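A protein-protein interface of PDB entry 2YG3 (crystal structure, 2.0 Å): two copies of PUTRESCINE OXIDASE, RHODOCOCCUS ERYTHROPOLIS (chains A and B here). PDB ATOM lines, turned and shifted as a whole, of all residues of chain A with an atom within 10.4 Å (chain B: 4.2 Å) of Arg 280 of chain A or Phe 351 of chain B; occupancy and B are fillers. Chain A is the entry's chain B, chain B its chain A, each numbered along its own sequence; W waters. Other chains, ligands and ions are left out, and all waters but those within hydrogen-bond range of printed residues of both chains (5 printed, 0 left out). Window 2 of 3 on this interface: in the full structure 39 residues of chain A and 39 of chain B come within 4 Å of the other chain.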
ATOM      1  N   TRP A 240      23.777   6.026  -4.726  1.00  0.00           N
ATOM      2  CA  TRP A 240      24.962   5.176  -4.750  1.00  0.00           C
ATOM      3  C   TRP A 240      24.657   3.699  -4.948  1.00  0.00           C
ATOM      4  O   TRP A 240      23.552   3.231  -4.651  1.00  0.00           O
ATOM      5  CB  TRP A 240      25.776   5.357  -3.465  1.00  0.00           C
ATOM      6  CG  TRP A 240      25.005   4.951  -2.225  1.00  0.00           C
ATOM      7  CD1 TRP A 240      24.011   5.659  -1.606  1.00  0.00           C
ATOM      8  CD2 TRP A 240      25.160   3.739  -1.476  1.00  0.00           C
ATOM      9  NE1 TRP A 240      23.534   4.962  -0.513  1.00  0.00           N
ATOM     10  CE2 TRP A 240      24.233   3.787  -0.405  1.00  0.00           C
ATOM     11  CE3 TRP A 240      25.997   2.622  -1.598  1.00  0.00           C
ATOM     12  CZ2 TRP A 240      24.111   2.748   0.525  1.00  0.00           C
ATOM     13  CZ3 TRP A 240      25.890   1.606  -0.669  1.00  0.00           C
ATOM     14  CH2 TRP A 240      24.952   1.668   0.376  1.00  0.00           C
ATOM     15  N   PRO A 276      20.261   4.310  -2.127  1.00  0.00           N
ATOM     16  CA  PRO A 276      19.378   3.893  -1.013  1.00  0.00           C
ATOM     17  C   PRO A 276      19.831   4.431   0.361  1.00  0.00           C
ATOM     18  O   PRO A 276      20.954   4.975   0.483  1.00  0.00           O
ATOM     19  CB  PRO A 276      19.502   2.369  -1.025  1.00  0.00           C
ATOM     20  CG  PRO A 276      20.965   2.133  -1.479  1.00  0.00           C
ATOM     21  CD  PRO A 276      21.197   3.233  -2.519  1.00  0.00           C
ATOM     22  N   PRO A 277      18.967   4.301   1.390  1.00  0.00           N
ATOM     23  CA  PRO A 277      19.357   4.767   2.736  1.00  0.00           C
ATOM     24  C   PRO A 277      20.647   4.128   3.231  1.00  0.00           C
ATOM     25  O   PRO A 277      21.021   3.030   2.782  1.00  0.00           O
ATOM     26  CB  PRO A 277      18.193   4.322   3.619  1.00  0.00           C
ATOM     27  CG  PRO A 277      17.024   4.208   2.700  1.00  0.00           C
ATOM     28  CD  PRO A 277      17.570   3.815   1.348  1.00  0.00           C
ATOM     29  N   LEU A 278      21.351   4.825   4.123  1.00  0.00           N
ATOM     30  CA  LEU A 278      22.513   4.243   4.773  1.00  0.00           C
ATOM     31  C   LEU A 278      22.059   3.038   5.607  1.00  0.00           C
ATOM     32  O   LEU A 278      20.890   2.988   6.012  1.00  0.00           O
ATOM     33  CB  LEU A 278      23.230   5.288   5.636  1.00  0.00           C
ATOM     34  CG  LEU A 278      23.829   6.490   4.886  1.00  0.00           C
ATOM     35  CD1 LEU A 278      24.614   7.379   5.861  1.00  0.00           C
ATOM     36  CD2 LEU A 278      24.744   6.033   3.733  1.00  0.00           C
ATOM     37  N   PRO A 279      22.960   2.062   5.850  1.00  0.00           N
ATOM     38  CA  PRO A 279      22.606   0.913   6.691  1.00  0.00           C
ATOM     39  C   PRO A 279      22.222   1.325   8.112  1.00  0.00           C
ATOM     40  O   PRO A 279      22.567   2.432   8.577  1.00  0.00           O
ATOM     41  CB  PRO A 279      23.885   0.069   6.703  1.00  0.00           C
ATOM     42  CG  PRO A 279      24.602   0.445   5.420  1.00  0.00           C
ATOM     43  CD  PRO A 279      24.306   1.914   5.257  1.00  0.00           C
ATOM     44  N   ARG A 280      21.521   0.437   8.810  1.00  0.00           N
ATOM     45  CA  ARG A 280      21.037   0.767  10.146  1.00  0.00           C
ATOM     46  C   ARG A 280      22.175   1.171  11.102  1.00  0.00           C
ATOM     47  O   ARG A 280      21.966   1.982  12.013  1.00  0.00           O
ATOM     48  CB  ARG A 280      20.218  -0.392  10.737  1.00  0.00           C
ATOM     49  CG  ARG A 280      21.045  -1.528  11.312  1.00  0.00           C
ATOM     50  CD  ARG A 280      20.209  -2.589  12.062  1.00  0.00           C
ATOM     51  NE  ARG A 280      19.481  -3.482  11.161  1.00  0.00           N
ATOM     52  CZ  ARG A 280      20.036  -4.462  10.460  1.00  0.00           C
ATOM     53  NH1 ARG A 280      21.288  -4.712  10.480  1.00  0.00           N
ATOM     54  NH2 ARG A 280      19.373  -5.219   9.683  1.00  0.00           N
ATOM     55  N   ARG A 281      23.360   0.587  10.907  1.00  0.00           N
ATOM     56  CA  ARG A 281      24.523   0.911  11.752  1.00  0.00           C
ATOM     57  C   ARG A 281      24.825   2.411  11.736  1.00  0.00           C
ATOM     58  O   ARG A 281      24.973   3.040  12.789  1.00  0.00           O
ATOM     59  CB  ARG A 281      25.761   0.116  11.301  1.00  0.00           C
ATOM     60  CG  ARG A 281      26.972   0.262  12.232  1.00  0.00           C
ATOM     61  CD  ARG A 281      26.578  -0.073  13.659  1.00  0.00           C
ATOM     62  NE  ARG A 281      27.737  -0.136  14.538  1.00  0.00           N
ATOM     63  CZ  ARG A 281      27.696  -0.415  15.839  1.00  0.00           C
ATOM     64  NH1 ARG A 281      26.545  -0.665  16.455  1.00  0.00           N
ATOM     65  NH2 ARG A 281      28.830  -0.454  16.519  1.00  0.00           N
ATOM     66  N   GLN A 282      24.889   2.977  10.540  1.00  0.00           N
ATOM     67  CA  GLN A 282      25.100   4.410  10.371  1.00  0.00           C
ATOM     68  C   GLN A 282      23.882   5.221  10.844  1.00  0.00           C
ATOM     69  O   GLN A 282      24.058   6.228  11.535  1.00  0.00           O
ATOM     70  CB  GLN A 282      25.467   4.729   8.924  1.00  0.00           C
ATOM     71  CG  GLN A 282      26.945   4.409   8.575  1.00  0.00           C
ATOM     72  CD  GLN A 282      27.260   2.916   8.513  1.00  0.00           C
ATOM     73  OE1 GLN A 282      26.405   2.094   8.180  1.00  0.00           O
ATOM     74  NE2 GLN A 282      28.504   2.563   8.821  1.00  0.00           N
ATOM     75  N   HIS A 283      22.664   4.780  10.495  1.00  0.00           N
ATOM     76  CA  HIS A 283      21.441   5.451  10.954  1.00  0.00           C
ATOM     77  C   HIS A 283      21.476   5.688  12.469  1.00  0.00           C
ATOM     78  O   HIS A 283      21.109   6.781  12.956  1.00  0.00           O
ATOM     79  CB  HIS A 283      20.196   4.608  10.642  1.00  0.00           C
ATOM     80  CG  HIS A 283      19.618   4.809   9.278  1.00  0.00           C
ATOM     81  ND1 HIS A 283      20.028   5.810   8.416  1.00  0.00           N
ATOM     82  CD2 HIS A 283      18.609   4.163   8.649  1.00  0.00           C
ATOM     83  CE1 HIS A 283      19.308   5.755   7.309  1.00  0.00           C
ATOM     84  NE2 HIS A 283      18.437   4.770   7.428  1.00  0.00           N
ATOM     85  N   GLN A 284      21.872   4.640  13.208  1.00  0.00           N
ATOM     86  CA  GLN A 284      21.934   4.668  14.670  1.00  0.00           C
ATOM     87  C   GLN A 284      23.156   5.418  15.200  1.00  0.00           C
ATOM     88  O   GLN A 284      23.018   6.338  16.010  1.00  0.00           O
ATOM     89  CB  GLN A 284      21.941   3.239  15.223  1.00  0.00           C
ATOM     90  CG  GLN A 284      20.550   2.605  15.278  1.00  0.00           C
ATOM     91  CD  GLN A 284      19.830   2.934  16.569  1.00  0.00           C
ATOM     92  OE1 GLN A 284      18.719   3.498  16.554  1.00  0.00           O
ATOM     93  NE2 GLN A 284      20.472   2.634  17.701  1.00  0.00           N
ATOM     94  N   MET A 285      24.345   5.031  14.732  1.00  0.00           N
ATOM     95  CA  MET A 285      25.595   5.683  15.143  1.00  0.00           C
ATOM     96  C   MET A 285      25.571   7.193  14.955  1.00  0.00           C
ATOM     97  O   MET A 285      26.012   7.926  15.834  1.00  0.00           O
ATOM     98  CB  MET A 285      26.802   5.079  14.394  1.00  0.00           C
ATOM     99  CG  MET A 285      28.068   5.912  14.487  1.00  0.00           C
ATOM    100  SD  MET A 285      29.505   5.047  13.801  1.00  0.00           S
ATOM    101  CE  MET A 285      28.920   4.805  12.111  1.00  0.00           C
ATOM    102  N   HIS A 286      25.084   7.663  13.807  1.00  0.00           N
ATOM    103  CA  HIS A 286      25.100   9.103  13.522  1.00  0.00           C
ATOM    104  C   HIS A 286      24.270   9.945  14.510  1.00  0.00           C
ATOM    105  O   HIS A 286      24.583  11.102  14.724  1.00  0.00           O
ATOM    106  CB  HIS A 286      24.707   9.412  12.067  1.00  0.00           C
ATOM    107  CG  HIS A 286      25.668   8.840  11.063  1.00  0.00           C
ATOM    108  ND1 HIS A 286      25.374   8.733   9.722  1.00  0.00           N
ATOM    109  CD2 HIS A 286      26.909   8.309  11.222  1.00  0.00           C
ATOM    110  CE1 HIS A 286      26.403   8.187   9.089  1.00  0.00           C
ATOM    111  NE2 HIS A 286      27.345   7.915   9.980  1.00  0.00           N
ATOM    112  N   GLN A 287      23.251   9.347  15.120  1.00  0.00           N
ATOM    113  CA  GLN A 287      22.394  10.094  16.056  1.00  0.00           C
ATOM    114  C   GLN A 287      23.111  10.333  17.381  1.00  0.00           C
ATOM    115  O   GLN A 287      22.695  11.179  18.176  1.00  0.00           O
ATOM    116  CB  GLN A 287      21.108   9.314  16.347  1.00  0.00           C
ATOM    117  CG  GLN A 287      20.141   9.152  15.162  1.00  0.00           C
ATOM    118  CD  GLN A 287      18.949   8.294  15.540  1.00  0.00           C
ATOM    119  OE1 GLN A 287      18.209   8.619  16.472  1.00  0.00           O
ATOM    120  NE2 GLN A 287      18.757   7.196  14.822  1.00  0.00           N
ATOM    121  N   HIS A 288      24.153   9.544  17.645  1.00  0.00           N
ATOM    122  CA  HIS A 288      24.834   9.588  18.926  1.00  0.00           C
ATOM    123  C   HIS A 288      26.065  10.497  18.896  1.00  0.00           C
ATOM    124  O   HIS A 288      26.841  10.485  19.822  1.00  0.00           O
ATOM    125  CB  HIS A 288      25.203   8.178  19.388  1.00  0.00           C
ATOM    126  CG  HIS A 288      24.019   7.341  19.778  1.00  0.00           C
ATOM    127  ND1 HIS A 288      23.450   7.393  21.031  1.00  0.00           N
ATOM    128  CD2 HIS A 288      23.286   6.453  19.068  1.00  0.00           C
ATOM    129  CE1 HIS A 288      22.425   6.558  21.085  1.00  0.00           C
ATOM    130  NE2 HIS A 288      22.307   5.969  19.905  1.00  0.00           N
ATOM    131  N   ARG A 406      30.689   1.859  22.065  1.00  0.00           N
ATOM    132  CA  ARG A 406      29.636   1.196  21.298  1.00  0.00           C
ATOM    133  C   ARG A 406      29.799   1.367  19.786  1.00  0.00           C
ATOM    134  O   ARG A 406      29.516   0.428  19.032  1.00  0.00           O
ATOM    135  CB  ARG A 406      28.281   1.746  21.731  1.00  0.00           C
ATOM    136  CG  ARG A 406      27.085   1.017  21.141  1.00  0.00           C
ATOM    137  CD  ARG A 406      25.780   1.468  21.840  1.00  0.00           C
ATOM    138  NE  ARG A 406      24.615   0.778  21.274  1.00  0.00           N
ATOM    139  CZ  ARG A 406      23.359   1.033  21.623  1.00  0.00           C
ATOM    140  NH1 ARG A 406      23.106   1.984  22.531  1.00  0.00           N
ATOM    141  NH2 ARG A 406      22.358   0.362  21.043  1.00  0.00           N
ATOM    142  N   TYR A 407      30.226   2.553  19.332  1.00  0.00           N
ATOM    143  CA  TYR A 407      30.205   2.864  17.883  1.00  0.00           C
ATOM    144  C   TYR A 407      31.567   3.209  17.303  1.00  0.00           C
ATOM    145  O   TYR A 407      31.729   3.246  16.069  1.00  0.00           O
ATOM    146  CB  TYR A 407      29.254   4.032  17.569  1.00  0.00           C
ATOM    147  CG  TYR A 407      27.826   3.786  17.966  1.00  0.00           C
ATOM    148  CD1 TYR A 407      27.057   2.822  17.298  1.00  0.00           C
ATOM    149  CD2 TYR A 407      27.239   4.504  19.011  1.00  0.00           C
ATOM    150  CE1 TYR A 407      25.750   2.592  17.646  1.00  0.00           C
ATOM    151  CE2 TYR A 407      25.904   4.277  19.383  1.00  0.00           C
ATOM    152  CZ  TYR A 407      25.178   3.315  18.682  1.00  0.00           C
ATOM    153  OH  TYR A 407      23.869   3.047  19.008  1.00  0.00           O
ATOM    154  N   ASP A 410      33.344   1.853  14.207  1.00  0.00           N
ATOM    155  CA  ASP A 410      32.662   1.987  12.917  1.00  0.00           C
ATOM    156  C   ASP A 410      32.646   3.430  12.399  1.00  0.00           C
ATOM    157  O   ASP A 410      32.106   3.698  11.320  1.00  0.00           O
ATOM    158  CB  ASP A 410      31.219   1.457  13.025  1.00  0.00           C
ATOM    159  CG  ASP A 410      31.166  -0.032  13.343  1.00  0.00           C
ATOM    160  OD1 ASP A 410      32.057  -0.773  12.912  1.00  0.00           O
ATOM    161  OD2 ASP A 410      30.229  -0.477  14.024  1.00  0.00           O
ATOM    162  N   VAL A 415      30.983   3.043   3.632  1.00  0.00           N
ATOM    163  CA  VAL A 415      29.762   2.353   3.251  1.00  0.00           C
ATOM    164  C   VAL A 415      29.802   2.291   1.725  1.00  0.00           C
ATOM    165  O   VAL A 415      29.487   3.264   1.038  1.00  0.00           O
ATOM    166  CB  VAL A 415      28.499   3.115   3.741  1.00  0.00           C
ATOM    167  CG1 VAL A 415      27.205   2.496   3.179  1.00  0.00           C
ATOM    168  CG2 VAL A 415      28.465   3.128   5.263  1.00  0.00           C
ATOM    169  N   ILE B 295      15.032  -4.808  18.960  1.00  0.00           N
ATOM    170  CA  ILE B 295      14.496  -5.735  17.978  1.00  0.00           C
ATOM    171  C   ILE B 295      13.210  -6.337  18.535  1.00  0.00           C
ATOM    172  O   ILE B 295      13.242  -7.063  19.536  1.00  0.00           O
ATOM    173  CB  ILE B 295      15.462  -6.884  17.638  1.00  0.00           C
ATOM    174  CG1 ILE B 295      16.853  -6.324  17.283  1.00  0.00           C
ATOM    175  CG2 ILE B 295      14.859  -7.747  16.506  1.00  0.00           C
ATOM    176  CD1 ILE B 295      17.922  -7.398  17.043  1.00  0.00           C
ATOM    177  N   ALA B 347      20.887  -5.791  21.069  1.00  0.00           N
ATOM    178  CA  ALA B 347      20.419  -5.662  19.684  1.00  0.00           C
ATOM    179  C   ALA B 347      21.605  -5.465  18.724  1.00  0.00           C
ATOM    180  O   ALA B 347      21.663  -6.098  17.660  1.00  0.00           O
ATOM    181  CB  ALA B 347      19.413  -4.497  19.554  1.00  0.00           C
ATOM    182  N   ASP B 348      22.549  -4.592  19.110  1.00  0.00           N
ATOM    183  CA  ASP B 348      23.767  -4.374  18.324  1.00  0.00           C
ATOM    184  C   ASP B 348      24.484  -5.705  18.114  1.00  0.00           C
ATOM    185  O   ASP B 348      24.924  -6.007  17.008  1.00  0.00           O
ATOM    186  CB  ASP B 348      24.755  -3.440  19.060  1.00  0.00           C
ATOM    187  CG  ASP B 348      24.318  -1.969  19.065  1.00  0.00           C
ATOM    188  OD1 ASP B 348      23.127  -1.677  18.836  1.00  0.00           O
ATOM    189  OD2 ASP B 348      25.190  -1.089  19.313  1.00  0.00           O
ATOM    190  N   ALA B 349      24.633  -6.465  19.198  1.00  0.00           N
ATOM    191  CA  ALA B 349      25.365  -7.727  19.134  1.00  0.00           C
ATOM    192  C   ALA B 349      24.660  -8.720  18.219  1.00  0.00           C
ATOM    193  O   ALA B 349      25.326  -9.446  17.476  1.00  0.00           O
ATOM    194  CB  ALA B 349      25.556  -8.317  20.527  1.00  0.00           C
ATOM    195  N   MET B 350      23.327  -8.740  18.260  1.00  0.00           N
ATOM    196  CA  MET B 350      22.559  -9.626  17.377  1.00  0.00           C
ATOM    197  C   MET B 350      22.714  -9.244  15.892  1.00  0.00           C
ATOM    198  O   MET B 350      22.926 -10.117  15.034  1.00  0.00           O
ATOM    199  CB  MET B 350      21.085  -9.701  17.814  1.00  0.00           C
ATOM    200  CG  MET B 350      20.855 -10.494  19.118  1.00  0.00           C
ATOM    201  SD  MET B 350      21.534 -12.193  19.101  1.00  0.00           S
ATOM    202  CE  MET B 350      23.083 -11.952  19.973  1.00  0.00           C
ATOM    203  N   PHE B 351      22.661  -7.941  15.605  1.00  0.00           N
ATOM    204  CA  PHE B 351      22.816  -7.449  14.232  1.00  0.00           C
ATOM    205  C   PHE B 351      24.235  -7.662  13.647  1.00  0.00           C
ATOM    206  O   PHE B 351      24.411  -7.653  12.430  1.00  0.00           O
ATOM    207  CB  PHE B 351      22.388  -5.980  14.132  1.00  0.00           C
ATOM    208  CG  PHE B 351      20.899  -5.774  14.120  1.00  0.00           C
ATOM    209  CD1 PHE B 351      20.082  -6.513  13.274  1.00  0.00           C
ATOM    210  CD2 PHE B 351      20.313  -4.794  14.932  1.00  0.00           C
ATOM    211  CE1 PHE B 351      18.694  -6.295  13.245  1.00  0.00           C
ATOM    212  CE2 PHE B 351      18.932  -4.575  14.899  1.00  0.00           C
ATOM    213  CZ  PHE B 351      18.124  -5.327  14.054  1.00  0.00           C
ATOM    214  N   GLU B 352      25.225  -7.873  14.509  1.00  0.00           N
ATOM    215  CA  GLU B 352      26.571  -8.291  14.055  1.00  0.00           C
ATOM    216  C   GLU B 352      26.602  -9.713  13.472  1.00  0.00           C
ATOM    217  O   GLU B 352      27.433 -10.018  12.626  1.00  0.00           O
ATOM    218  CB  GLU B 352      27.568  -8.229  15.203  1.00  0.00           C
ATOM    219  CG  GLU B 352      27.984  -6.823  15.591  1.00  0.00           C
ATOM    220  CD  GLU B 352      28.930  -6.823  16.780  1.00  0.00           C
ATOM    221  OE1 GLU B 352      29.838  -7.689  16.826  1.00  0.00           O
ATOM    222  OE2 GLU B 352      28.762  -5.975  17.685  1.00  0.00           O
ATOM    223  N   LEU B 353      25.703 -10.574  13.942  1.00  0.00           N
ATOM    224  CA  LEU B 353      25.605 -11.939  13.444  1.00  0.00           C
ATOM    225  C   LEU B 353      24.893 -11.972  12.105  1.00  0.00           C
ATOM    226  O   LEU B 353      24.142 -11.048  11.770  1.00  0.00           O
ATOM    227  CB  LEU B 353      24.842 -12.793  14.444  1.00  0.00           C
ATOM    228  CG  LEU B 353      25.347 -12.838  15.887  1.00  0.00           C
ATOM    229  CD1 LEU B 353      24.383 -13.638  16.755  1.00  0.00           C
ATOM    230  CD2 LEU B 353      26.769 -13.431  15.957  1.00  0.00           C
ATOM    231  N   ARG B 358      21.670 -15.065  14.102  1.00  0.00           N
ATOM    232  CA  ARG B 358      20.842 -14.214  14.973  1.00  0.00           C
ATOM    233  C   ARG B 358      19.504 -14.898  15.281  1.00  0.00           C
ATOM    234  O   ARG B 358      19.105 -14.975  16.439  1.00  0.00           O
ATOM    235  CB  ARG B 358      20.631 -12.845  14.308  1.00  0.00           C
ATOM    236  CG  ARG B 358      19.578 -11.923  14.993  1.00  0.00           C
ATOM    237  CD  ARG B 358      19.654 -10.485  14.468  1.00  0.00           C
ATOM    238  NE  ARG B 358      19.247 -10.346  13.080  1.00  0.00           N
ATOM    239  CZ  ARG B 358      20.066 -10.192  12.046  1.00  0.00           C
ATOM    240  NH1 ARG B 358      21.376 -10.145  12.224  1.00  0.00           N
ATOM    241  NH2 ARG B 358      19.556 -10.079  10.824  1.00  0.00           N
ATOM    242  N   ASP B 384      12.637  -4.162  12.004  1.00  0.00           N
ATOM    243  CA  ASP B 384      13.957  -3.572  11.802  1.00  0.00           C
ATOM    244  C   ASP B 384      13.780  -2.059  11.583  1.00  0.00           C
ATOM    245  O   ASP B 384      14.023  -1.531  10.499  1.00  0.00           O
ATOM    246  CB  ASP B 384      14.632  -4.266  10.596  1.00  0.00           C
ATOM    247  CG  ASP B 384      16.073  -3.786  10.338  1.00  0.00           C
ATOM    248  OD1 ASP B 384      16.717  -3.212  11.256  1.00  0.00           O
ATOM    249  OD2 ASP B 384      16.552  -3.982   9.199  1.00  0.00           O
ATOM    250  N   GLY B 386      15.528   0.413  12.794  1.00  0.00           N
ATOM    251  CA  GLY B 386      16.833   1.078  12.540  1.00  0.00           C
ATOM    252  C   GLY B 386      17.146   1.284  11.063  1.00  0.00           C
ATOM    253  O   GLY B 386      17.762   2.309  10.667  1.00  0.00           O
ATOM    254  N   SER B 387      16.723   0.333  10.229  1.00  0.00           N
ATOM    255  CA  SER B 387      16.954   0.421   8.779  1.00  0.00           C
ATOM    256  C   SER B 387      16.064   1.433   8.069  1.00  0.00           C
ATOM    257  O   SER B 387      16.403   1.905   6.973  1.00  0.00           O
ATOM    258  CB  SER B 387      16.823  -0.950   8.107  1.00  0.00           C
ATOM    259  OG  SER B 387      17.886  -1.797   8.500  1.00  0.00           O
HETATM  260  O   HOH W   1      27.942  -3.719  16.864  1.00  0.00           O
HETATM  261  O   HOH W   2      20.309  -1.737   7.274  1.00  0.00           O
HETATM  262  O   HOH W   3      22.716   0.933  17.650  1.00  0.00           O
HETATM  263  O   HOH W   4      27.692  -1.671  18.988  1.00  0.00           O
HETATM  264  O   HOH W   5      18.719   1.271   5.909  1.00  0.00           O
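The side-chain carboxylate of Asp 348 of chain B lies within salt-bridge range of the guanidinium group of Arg 406 of chain A, at 2.8 Å.
OD1 of Asp 384 of chain B lies within salt-bridge range of NE of Arg 280 of chain A.
OD2 of Asp 348 of chain B lies within salt-bridge range of NH1 of Arg 281 of chain A.
OG of Ser 387 of chain B sits at hydrogen-bond distance from OD2 of Asp 384 of chain B (2.7 Å).
NE2 of Gln 287 of chain A sits at hydrogen-bond distance from O of His 283 of chain A (3.0 Å).
The guanidinium group of Arg 406 of chain A sits at hydrogen-bond distance from the side-chain hydroxyl of Tyr 407 of chain A (3.3 Å).
The guanidinium group (NE) of Arg 281 of chain A lies within salt-bridge range of the side-chain carboxylate (OD2) of Asp 410 of chain A, 2.6 Å away.
NH2 of Arg 281 of chain A is in hydrogen-bond range of O of Arg 406 of chain A (2.8 Å).
A ring nitrogen (NE2) of His 283 of chain A is in hydrogen-bond range of the backbone carbonyl oxygen of Leu 278 of chain A, at 3.3 Å.
Printed residues of chain B that touch a printed residue of chain A: Asp 348, Phe 351, Asp 384, Gly 386 and Ser 387.
Arg 280 of chain A touches just these residues of chain B: Phe 351 (3.5 Å), Asp 384 (2.8 Å), Gly 386 (3.5 Å) and Ser 387 (3.5 Å).
Phe 351 of chain B touches just one residue of chain A: Arg 280.
Asp 384 of chain B touches one residue of chain A.
Of chain A, only Arg 280 and His 283 come within 4 Å of Gly 386 of chain B.
Ser 387 of chain B touches just these residues of chain A: Arg 280 and His 283.
Of the printed residues of chain A, Asp 348 of chain B touches Arg 281 and Arg 406.
Of the printed residues of chain B, His 283 of chain A touches Gly 386 (2.9 Å) and Ser 387 (3.5 Å).
Printed residues of chain B within 4 Å of Arg 281 of chain A: Asp 348 (3.2 Å).
Of the printed residues of chain B, Arg 406 of chain A touches Asp 348 (2.8 Å).
Gln 282 of chain A touches none of the printed residues of chain B.
The nearest printed residue of chain B that does not touch Arg 281 of chain A is Glu 352 of chain B (5.6 Å).
Arg 280 of chain A touches Phe 351 of chain B (CZ to CD1, 3.5 Å).
Gly 386 of chain B touches Arg 280 of chain A (C to CB, 3.5 Å).
OG of Ser 387 of chain B touches CB of Arg 280 of chain A, 3.5 Å away.
His 283 of chain A touches Gly 386 of chain B.
NE2 of His 283 of chain A touches O of Ser 387 of chain B, 3.5 Å away.
No position is printed for both chains.
Water W1 lies within hydrogen-bond range of the side-chain carboxylate of Glu 352 of chain B (2.5 Å) and the guanidinium group of Arg 281 of chain A (3.4 Å).
Water W4 lies within hydrogen-bond range of the side-chain carboxylate (OD2) of Asp 348 of chain B (2.6 Å), the backbone carbonyl oxygen (O) of Arg 406 of chain A (2.8 Å) and the guanidinium group (NH1) of Arg 281 of chain A (3.0 Å).
Water W5 lies within hydrogen-bond range of the backbone carbonyl oxygen of Ser 387 of chain B (2.6 Å) and the backbone carbonyl oxygen of Leu 278 of chain A (2.8 Å).
Water W2 lies within hydrogen-bond range of the side-chain hydroxyl of Ser 387 of chain B (2.7 Å) and the backbone NH of Arg 280 of chain A (2.9 Å).
Water W3 lies within hydrogen-bond range of OH of Tyr 407 of chain A (2.8 Å), NE2 of Gln 284 of chain A (2.8 Å), OD1 of Asp 348 of chain B (2.9 Å) and NH2 of Arg 406 of chain A (3.5 Å).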
